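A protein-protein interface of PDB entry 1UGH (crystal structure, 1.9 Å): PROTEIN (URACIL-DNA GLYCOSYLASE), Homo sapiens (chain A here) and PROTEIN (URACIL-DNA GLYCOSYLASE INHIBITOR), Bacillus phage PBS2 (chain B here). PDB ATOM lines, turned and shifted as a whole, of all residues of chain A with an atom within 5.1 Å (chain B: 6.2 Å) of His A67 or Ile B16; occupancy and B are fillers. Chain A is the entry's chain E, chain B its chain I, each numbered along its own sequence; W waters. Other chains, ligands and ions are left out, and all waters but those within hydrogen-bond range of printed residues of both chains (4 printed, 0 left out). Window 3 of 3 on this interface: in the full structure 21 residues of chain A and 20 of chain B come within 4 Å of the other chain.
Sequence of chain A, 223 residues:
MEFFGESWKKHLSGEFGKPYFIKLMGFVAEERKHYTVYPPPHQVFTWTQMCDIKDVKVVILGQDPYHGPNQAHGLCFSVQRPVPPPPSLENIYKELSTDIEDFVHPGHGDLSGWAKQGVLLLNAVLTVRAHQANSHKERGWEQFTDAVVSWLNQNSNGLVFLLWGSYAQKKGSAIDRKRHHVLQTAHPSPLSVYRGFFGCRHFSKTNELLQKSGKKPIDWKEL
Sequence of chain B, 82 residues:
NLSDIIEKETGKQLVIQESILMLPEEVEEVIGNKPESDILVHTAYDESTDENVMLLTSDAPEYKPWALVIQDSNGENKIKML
His A67 touches two residues of chain B.
Pro A69 touches none of the printed residues of chain B.
Of the printed residues of chain B, Gln A71 touches Gln B17.
Printed residues of chain B within 4 Å of Ala A133: Ser B19 (3.4 Å).
Of chain A, only His A67 (3.8 Å) comes within 4 Å of Ile B16.
The nearest residue of chain B that does not touch His A67 is Glu B18 (4.7 Å).
Among the printed residues, pairs that only touch across the chains: Tyr A66 with Gln B17 (3.3 Å), Ala A133 with Ser B19 (3.4 Å), His A67 with Ile B16 (3.8 Å) and Tyr A66 with Glu B18 (3.8 Å).
Water W1 lies within hydrogen-bond range of O of Ile B16 and OE1 of Gln A71.
Water W4 lies within hydrogen-bond range of OH of Tyr A66 (2.6 Å) and OE1 of Glu B18 (2.7 Å).
Water W2 lies within hydrogen-bond range of the side-chain amide oxygen (OE1) of Gln A71 (2.9 Å), the backbone carbonyl oxygen (O) of Gln B17 (3.2 Å) and a ring nitrogen (ND1) of His A67 (3.3 Å).
Water W3 bridges the side-chain amide nitrogen of Gln A71 and the side-chain amide nitrogen of Gln B17.
O of His A67 lies within hydrogen-bond range of N of His A131.
OE1 of Gln A71 lies close to N of Gly A68 (3.4 Å).
The backbone carbonyl oxygen (O) of Thr B43 is in hydrogen-bond range of the backbone NH (N) of Gln B17.
The backbone NH (N) of Thr B43 is in hydrogen-bond range of the backbone carbonyl oxygen (O) of Glu B18 (2.8 Å).
Of the 14 printed residues of chain B, 4 touch a printed residue of chain A.
Among the printed residues, 6 pairs touch across the chains.
NE2 of His A67 sits at hydrogen-bond distance from OG of Ser B19.
The side-chain amide nitrogen (NE2) of Gln A71 lies within hydrogen-bond range of the backbone carbonyl oxygen (O) of Gln B17 (3.1 Å).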
ATOM      1  N   TYR A  38      14.791  29.120  -8.217  1.00  0.00           N
ATOM      2  CA  TYR A  38      13.730  28.163  -8.496  1.00  0.00           C
ATOM      3  C   TYR A  38      12.446  28.564  -7.751  1.00  0.00           C
ATOM      4  O   TYR A  38      12.517  29.036  -6.613  1.00  0.00           O
ATOM      5  CB  TYR A  38      14.182  26.774  -8.042  1.00  0.00           C
ATOM      6  CG  TYR A  38      15.397  26.256  -8.768  1.00  0.00           C
ATOM      7  CD1 TYR A  38      15.467  26.291 -10.162  1.00  0.00           C
ATOM      8  CD2 TYR A  38      16.469  25.707  -8.068  1.00  0.00           C
ATOM      9  CE1 TYR A  38      16.578  25.784 -10.847  1.00  0.00           C
ATOM     10  CE2 TYR A  38      17.579  25.194  -8.738  1.00  0.00           C
ATOM     11  CZ  TYR A  38      17.629  25.237 -10.127  1.00  0.00           C
ATOM     12  OH  TYR A  38      18.722  24.721 -10.769  1.00  0.00           O
ATOM     13  N   PRO A  65      10.727  25.783  -1.845  1.00  0.00           N
ATOM     14  CA  PRO A  65      10.849  24.907  -3.015  1.00  0.00           C
ATOM     15  C   PRO A  65      12.113  24.057  -3.045  1.00  0.00           C
ATOM     16  O   PRO A  65      13.073  24.325  -2.323  1.00  0.00           O
ATOM     17  CB  PRO A  65      10.833  25.887  -4.186  1.00  0.00           C
ATOM     18  CG  PRO A  65      10.226  27.142  -3.615  1.00  0.00           C
ATOM     19  CD  PRO A  65      10.818  27.196  -2.254  1.00  0.00           C
ATOM     20  N   TYR A  66      12.097  23.023  -3.888  1.00  0.00           N
ATOM     21  CA  TYR A  66      13.250  22.137  -4.047  1.00  0.00           C
ATOM     22  C   TYR A  66      14.344  22.961  -4.712  1.00  0.00           C
ATOM     23  O   TYR A  66      14.143  23.520  -5.799  1.00  0.00           O
ATOM     24  CB  TYR A  66      12.898  20.950  -4.938  1.00  0.00           C
ATOM     25  CG  TYR A  66      12.000  19.932  -4.283  1.00  0.00           C
ATOM     26  CD1 TYR A  66      12.472  19.123  -3.246  1.00  0.00           C
ATOM     27  CD2 TYR A  66      10.682  19.763  -4.709  1.00  0.00           C
ATOM     28  CE1 TYR A  66      11.651  18.170  -2.647  1.00  0.00           C
ATOM     29  CE2 TYR A  66       9.856  18.818  -4.120  1.00  0.00           C
ATOM     30  CZ  TYR A  66      10.343  18.023  -3.085  1.00  0.00           C
ATOM     31  OH  TYR A  66       9.507  17.108  -2.475  1.00  0.00           O
ATOM     32  N   HIS A  67      15.512  23.007  -4.074  1.00  0.00           N
ATOM     33  CA  HIS A  67      16.632  23.802  -4.573  1.00  0.00           C
ATOM     34  C   HIS A  67      17.543  23.147  -5.600  1.00  0.00           C
ATOM     35  O   HIS A  67      18.745  23.423  -5.622  1.00  0.00           O
ATOM     36  CB  HIS A  67      17.458  24.314  -3.397  1.00  0.00           C
ATOM     37  CG  HIS A  67      17.815  23.258  -2.395  1.00  0.00           C
ATOM     38  ND1 HIS A  67      18.594  22.161  -2.703  1.00  0.00           N
ATOM     39  CD2 HIS A  67      17.534  23.158  -1.075  1.00  0.00           C
ATOM     40  CE1 HIS A  67      18.780  21.436  -1.613  1.00  0.00           C
ATOM     41  NE2 HIS A  67      18.149  22.018  -0.611  1.00  0.00           N
ATOM     42  N   GLY A  68      16.966  22.346  -6.490  1.00  0.00           N
ATOM     43  CA  GLY A  68      17.758  21.662  -7.496  1.00  0.00           C
ATOM     44  C   GLY A  68      17.062  21.736  -8.831  1.00  0.00           C
ATOM     45  O   GLY A  68      15.834  21.827  -8.880  1.00  0.00           O
ATOM     46  N   PRO A  69      17.813  21.693  -9.936  1.00  0.00           N
ATOM     47  CA  PRO A  69      17.281  21.762 -11.301  1.00  0.00           C
ATOM     48  C   PRO A  69      16.238  20.710 -11.660  1.00  0.00           C
ATOM     49  O   PRO A  69      16.374  19.537 -11.302  1.00  0.00           O
ATOM     50  CB  PRO A  69      18.537  21.630 -12.162  1.00  0.00           C
ATOM     51  CG  PRO A  69      19.473  20.863 -11.290  1.00  0.00           C
ATOM     52  CD  PRO A  69      19.270  21.508  -9.957  1.00  0.00           C
ATOM     53  N   GLN A  71      13.322  20.155 -10.508  1.00  0.00           N
ATOM     54  CA  GLN A  71      12.428  19.680  -9.457  1.00  0.00           C
ATOM     55  C   GLN A  71      11.209  20.574  -9.232  1.00  0.00           C
ATOM     56  O   GLN A  71      10.128  20.325  -9.778  1.00  0.00           O
ATOM     57  CB  GLN A  71      13.190  19.494  -8.137  1.00  0.00           C
ATOM     58  CG  GLN A  71      14.150  18.306  -8.079  1.00  0.00           C
ATOM     59  CD  GLN A  71      14.905  18.247  -6.757  1.00  0.00           C
ATOM     60  OE1 GLN A  71      15.666  19.156  -6.428  1.00  0.00           O
ATOM     61  NE2 GLN A  71      14.703  17.179  -5.997  1.00  0.00           N
ATOM     62  N   VAL A 128      13.473  29.909  -4.011  1.00  0.00           N
ATOM     63  CA  VAL A 128      14.722  29.555  -3.351  1.00  0.00           C
ATOM     64  C   VAL A 128      15.833  29.718  -4.392  1.00  0.00           C
ATOM     65  O   VAL A 128      15.572  29.632  -5.599  1.00  0.00           O
ATOM     66  CB  VAL A 128      14.670  28.081  -2.861  1.00  0.00           C
ATOM     67  CG1 VAL A 128      14.592  27.117  -4.050  1.00  0.00           C
ATOM     68  CG2 VAL A 128      15.854  27.768  -1.974  1.00  0.00           C
ATOM     69  N   ARG A 129      17.048  30.035  -3.951  1.00  0.00           N
ATOM     70  CA  ARG A 129      18.153  30.164  -4.904  1.00  0.00           C
ATOM     71  C   ARG A 129      18.883  28.816  -4.980  1.00  0.00           C
ATOM     72  O   ARG A 129      19.254  28.235  -3.946  1.00  0.00           O
ATOM     73  CB  ARG A 129      19.085  31.332  -4.553  1.00  0.00           C
ATOM     74  CG  ARG A 129      19.600  31.376  -3.140  1.00  0.00           C
ATOM     75  CD  ARG A 129      19.923  32.819  -2.765  1.00  0.00           C
ATOM     76  NE  ARG A 129      21.033  32.948  -1.814  1.00  0.00           N
ATOM     77  CZ  ARG A 129      21.338  34.064  -1.155  1.00  0.00           C
ATOM     78  NH1 ARG A 129      20.612  35.154  -1.347  1.00  0.00           N
ATOM     79  NH2 ARG A 129      22.386  34.098  -0.325  1.00  0.00           N
ATOM     80  N   ALA A 130      18.932  28.273  -6.198  1.00  0.00           N
ATOM     81  CA  ALA A 130      19.548  26.981  -6.517  1.00  0.00           C
ATOM     82  C   ALA A 130      20.671  26.513  -5.592  1.00  0.00           C
ATOM     83  O   ALA A 130      21.750  27.092  -5.593  1.00  0.00           O
ATOM     84  CB  ALA A 130      20.044  26.996  -7.962  1.00  0.00           C
ATOM     85  N   HIS A 131      20.416  25.440  -4.844  1.00  0.00           N
ATOM     86  CA  HIS A 131      21.370  24.822  -3.911  1.00  0.00           C
ATOM     87  C   HIS A 131      21.444  25.356  -2.491  1.00  0.00           C
ATOM     88  O   HIS A 131      22.217  24.843  -1.683  1.00  0.00           O
ATOM     89  CB  HIS A 131      22.778  24.741  -4.498  1.00  0.00           C
ATOM     90  CG  HIS A 131      22.832  24.080  -5.840  1.00  0.00           C
ATOM     91  ND1 HIS A 131      22.398  22.788  -6.057  1.00  0.00           N
ATOM     92  CD2 HIS A 131      23.234  24.548  -7.044  1.00  0.00           C
ATOM     93  CE1 HIS A 131      22.529  22.491  -7.337  1.00  0.00           C
ATOM     94  NE2 HIS A 131      23.032  23.542  -7.959  1.00  0.00           N
ATOM     95  N   GLN A 132      20.654  26.371  -2.169  1.00  0.00           N
ATOM     96  CA  GLN A 132      20.650  26.904  -0.811  1.00  0.00           C
ATOM     97  C   GLN A 132      19.246  26.808  -0.208  1.00  0.00           C
ATOM     98  O   GLN A 132      18.380  27.641  -0.481  1.00  0.00           O
ATOM     99  CB  GLN A 132      21.127  28.353  -0.788  1.00  0.00           C
ATOM    100  CG  GLN A 132      22.602  28.554  -1.107  1.00  0.00           C
ATOM    101  CD  GLN A 132      23.044  29.996  -0.901  1.00  0.00           C
ATOM    102  OE1 GLN A 132      23.013  30.811  -1.827  1.00  0.00           O
ATOM    103  NE2 GLN A 132      23.420  30.328   0.330  1.00  0.00           N
ATOM    104  N   ALA A 133      19.025  25.784   0.607  1.00  0.00           N
ATOM    105  CA  ALA A 133      17.726  25.577   1.232  1.00  0.00           C
ATOM    106  C   ALA A 133      17.396  26.695   2.199  1.00  0.00           C
ATOM    107  O   ALA A 133      18.272  27.211   2.884  1.00  0.00           O
ATOM    108  CB  ALA A 133      17.696  24.246   1.957  1.00  0.00           C
ATOM    109  N   LEU B   2      27.569  21.164   1.103  1.00  0.00           N
ATOM    110  CA  LEU B   2      27.109  20.128   2.023  1.00  0.00           C
ATOM    111  C   LEU B   2      27.237  18.715   1.442  1.00  0.00           C
ATOM    112  O   LEU B   2      27.419  17.751   2.185  1.00  0.00           O
ATOM    113  CB  LEU B   2      25.674  20.416   2.466  1.00  0.00           C
ATOM    114  CG  LEU B   2      25.490  21.216   3.766  1.00  0.00           C
ATOM    115  CD1 LEU B   2      26.362  22.458   3.808  1.00  0.00           C
ATOM    116  CD2 LEU B   2      24.038  21.589   3.921  1.00  0.00           C
ATOM    117  N   SER B   3      27.187  18.606   0.117  1.00  0.00           N
ATOM    118  CA  SER B   3      27.291  17.314  -0.558  1.00  0.00           C
ATOM    119  C   SER B   3      28.663  16.678  -0.362  1.00  0.00           C
ATOM    120  O   SER B   3      28.765  15.495  -0.034  1.00  0.00           O
ATOM    121  CB  SER B   3      26.995  17.477  -2.048  1.00  0.00           C
ATOM    122  OG  SER B   3      27.733  18.558  -2.591  1.00  0.00           O
ATOM    123  N   ILE B   6      29.122  15.210   2.843  1.00  0.00           N
ATOM    124  CA  ILE B   6      28.548  13.865   2.897  1.00  0.00           C
ATOM    125  C   ILE B   6      29.504  12.838   2.273  1.00  0.00           C
ATOM    126  O   ILE B   6      29.757  11.787   2.856  1.00  0.00           O
ATOM    127  CB  ILE B   6      27.152  13.834   2.217  1.00  0.00           C
ATOM    128  CG1 ILE B   6      26.139  14.581   3.098  1.00  0.00           C
ATOM    129  CG2 ILE B   6      26.705  12.398   1.959  1.00  0.00           C
ATOM    130  CD1 ILE B   6      24.753  14.683   2.526  1.00  0.00           C
ATOM    131  N   LEU B  14      26.742  11.789  -2.893  1.00  0.00           N
ATOM    132  CA  LEU B  14      25.286  11.758  -2.910  1.00  0.00           C
ATOM    133  C   LEU B  14      24.640  13.068  -3.321  1.00  0.00           C
ATOM    134  O   LEU B  14      25.190  14.145  -3.082  1.00  0.00           O
ATOM    135  CB  LEU B  14      24.738  11.282  -1.564  1.00  0.00           C
ATOM    136  CG  LEU B  14      24.855   9.770  -1.377  1.00  0.00           C
ATOM    137  CD1 LEU B  14      24.496   9.391   0.025  1.00  0.00           C
ATOM    138  CD2 LEU B  14      23.962   9.054  -2.376  1.00  0.00           C
ATOM    139  N   VAL B  15      23.474  12.955  -3.957  1.00  0.00           N
ATOM    140  CA  VAL B  15      22.704  14.101  -4.429  1.00  0.00           C
ATOM    141  C   VAL B  15      21.604  14.422  -3.421  1.00  0.00           C
ATOM    142  O   VAL B  15      20.810  13.553  -3.083  1.00  0.00           O
ATOM    143  CB  VAL B  15      22.036  13.790  -5.795  1.00  0.00           C
ATOM    144  CG1 VAL B  15      21.339  15.022  -6.348  1.00  0.00           C
ATOM    145  CG2 VAL B  15      23.070  13.270  -6.782  1.00  0.00           C
ATOM    146  N   ILE B  16      21.580  15.654  -2.923  1.00  0.00           N
ATOM    147  CA  ILE B  16      20.560  16.078  -1.967  1.00  0.00           C
ATOM    148  C   ILE B  16      19.251  16.264  -2.719  1.00  0.00           C
ATOM    149  O   ILE B  16      19.154  17.118  -3.597  1.00  0.00           O
ATOM    150  CB  ILE B  16      20.918  17.418  -1.300  1.00  0.00           C
ATOM    151  CG1 ILE B  16      22.180  17.263  -0.446  1.00  0.00           C
ATOM    152  CG2 ILE B  16      19.749  17.919  -0.458  1.00  0.00           C
ATOM    153  CD1 ILE B  16      22.005  16.369   0.764  1.00  0.00           C
ATOM    154  N   GLN B  17      18.252  15.459  -2.372  1.00  0.00           N
ATOM    155  CA  GLN B  17      16.944  15.517  -3.015  1.00  0.00           C
ATOM    156  C   GLN B  17      16.005  16.511  -2.340  1.00  0.00           C
ATOM    157  O   GLN B  17      15.072  17.033  -2.972  1.00  0.00           O
ATOM    158  CB  GLN B  17      16.301  14.133  -3.008  1.00  0.00           C
ATOM    159  CG  GLN B  17      17.060  13.072  -3.800  1.00  0.00           C
ATOM    160  CD  GLN B  17      16.898  13.214  -5.307  1.00  0.00           C
ATOM    161  OE1 GLN B  17      17.400  14.160  -5.922  1.00  0.00           O
ATOM    162  NE2 GLN B  17      16.183  12.274  -5.909  1.00  0.00           N
ATOM    163  N   GLU B  18      16.264  16.787  -1.065  1.00  0.00           N
ATOM    164  CA  GLU B  18      15.421  17.695  -0.295  1.00  0.00           C
ATOM    165  C   GLU B  18      16.116  18.128   1.003  1.00  0.00           C
ATOM    166  O   GLU B  18      17.098  17.504   1.433  1.00  0.00           O
ATOM    167  CB  GLU B  18      14.114  16.971   0.052  1.00  0.00           C
ATOM    168  CG  GLU B  18      14.362  15.670   0.819  1.00  0.00           C
ATOM    169  CD  GLU B  18      13.112  14.873   1.107  1.00  0.00           C
ATOM    170  OE1 GLU B  18      12.285  14.698   0.196  1.00  0.00           O
ATOM    171  OE2 GLU B  18      12.961  14.389   2.239  1.00  0.00           O
ATOM    172  N   SER B  19      15.632  19.224   1.585  1.00  0.00           N
ATOM    173  CA  SER B  19      16.135  19.757   2.851  1.00  0.00           C
ATOM    174  C   SER B  19      14.887  20.195   3.599  1.00  0.00           C
ATOM    175  O   SER B  19      14.189  21.114   3.169  1.00  0.00           O
ATOM    176  CB  SER B  19      17.060  20.954   2.627  1.00  0.00           C
ATOM    177  OG  SER B  19      18.146  20.606   1.790  1.00  0.00           O
ATOM    178  N   HIS B  42      18.923  17.656   5.421  1.00  0.00           N
ATOM    179  CA  HIS B  42      19.297  17.504   4.024  1.00  0.00           C
ATOM    180  C   HIS B  42      19.353  16.004   3.756  1.00  0.00           C
ATOM    181  O   HIS B  42      20.217  15.309   4.290  1.00  0.00           O
ATOM    182  CB  HIS B  42      20.675  18.130   3.786  1.00  0.00           C
ATOM    183  CG  HIS B  42      20.763  19.561   4.208  1.00  0.00           C
ATOM    184  ND1 HIS B  42      21.024  19.939   5.508  1.00  0.00           N
ATOM    185  CD2 HIS B  42      20.600  20.706   3.508  1.00  0.00           C
ATOM    186  CE1 HIS B  42      21.014  21.259   5.590  1.00  0.00           C
ATOM    187  NE2 HIS B  42      20.760  21.747   4.390  1.00  0.00           N
ATOM    188  N   THR B  43      18.446  15.514   2.918  1.00  0.00           N
ATOM    189  CA  THR B  43      18.365  14.091   2.621  1.00  0.00           C
ATOM    190  C   THR B  43      18.701  13.720   1.184  1.00  0.00           C
ATOM    191  O   THR B  43      18.251  14.366   0.235  1.00  0.00           O
ATOM    192  CB  THR B  43      16.945  13.568   2.921  1.00  0.00           C
ATOM    193  OG1 THR B  43      16.494  14.113   4.167  1.00  0.00           O
ATOM    194  CG2 THR B  43      16.936  12.044   3.004  1.00  0.00           C
ATOM    195  N   ALA B  44      19.484  12.659   1.046  1.00  0.00           N
ATOM    196  CA  ALA B  44      19.875  12.121  -0.249  1.00  0.00           C
ATOM    197  C   ALA B  44      19.608  10.627  -0.100  1.00  0.00           C
ATOM    198  O   ALA B  44      19.639  10.105   1.024  1.00  0.00           O
ATOM    199  CB  ALA B  44      21.354  12.380  -0.515  1.00  0.00           C
ATOM    200  N   VAL B  53      20.522   8.850   3.577  1.00  0.00           N
ATOM    201  CA  VAL B  53      21.619   9.565   4.217  1.00  0.00           C
ATOM    202  C   VAL B  53      21.135  10.993   4.469  1.00  0.00           C
ATOM    203  O   VAL B  53      20.684  11.682   3.544  1.00  0.00           O
ATOM    204  CB  VAL B  53      22.841   9.579   3.297  1.00  0.00           C
ATOM    205  CG1 VAL B  53      24.061  10.045   4.052  1.00  0.00           C
ATOM    206  CG2 VAL B  53      23.059   8.197   2.712  1.00  0.00           C
ATOM    207  N   LEU B  55      22.129  14.715   6.216  1.00  0.00           N
ATOM    208  CA  LEU B  55      23.083  15.614   6.831  1.00  0.00           C
ATOM    209  C   LEU B  55      22.248  16.697   7.503  1.00  0.00           C
ATOM    210  O   LEU B  55      21.520  17.427   6.832  1.00  0.00           O
ATOM    211  CB  LEU B  55      24.007  16.198   5.757  1.00  0.00           C
ATOM    212  CG  LEU B  55      24.962  17.344   6.111  1.00  0.00           C
ATOM    213  CD1 LEU B  55      25.764  17.056   7.375  1.00  0.00           C
ATOM    214  CD2 LEU B  55      25.884  17.573   4.931  1.00  0.00           C
HETATM  215  O   HOH W   1      18.939  18.765  -5.640  1.00  0.00           O
HETATM  216  O   HOH W   2      16.513  19.806  -3.751  1.00  0.00           O
HETATM  217  O   HOH W   3      14.426  14.475  -7.055  1.00  0.00           O
HETATM  218  O   HOH W   4      10.480  16.678  -0.058  1.00  0.00           O
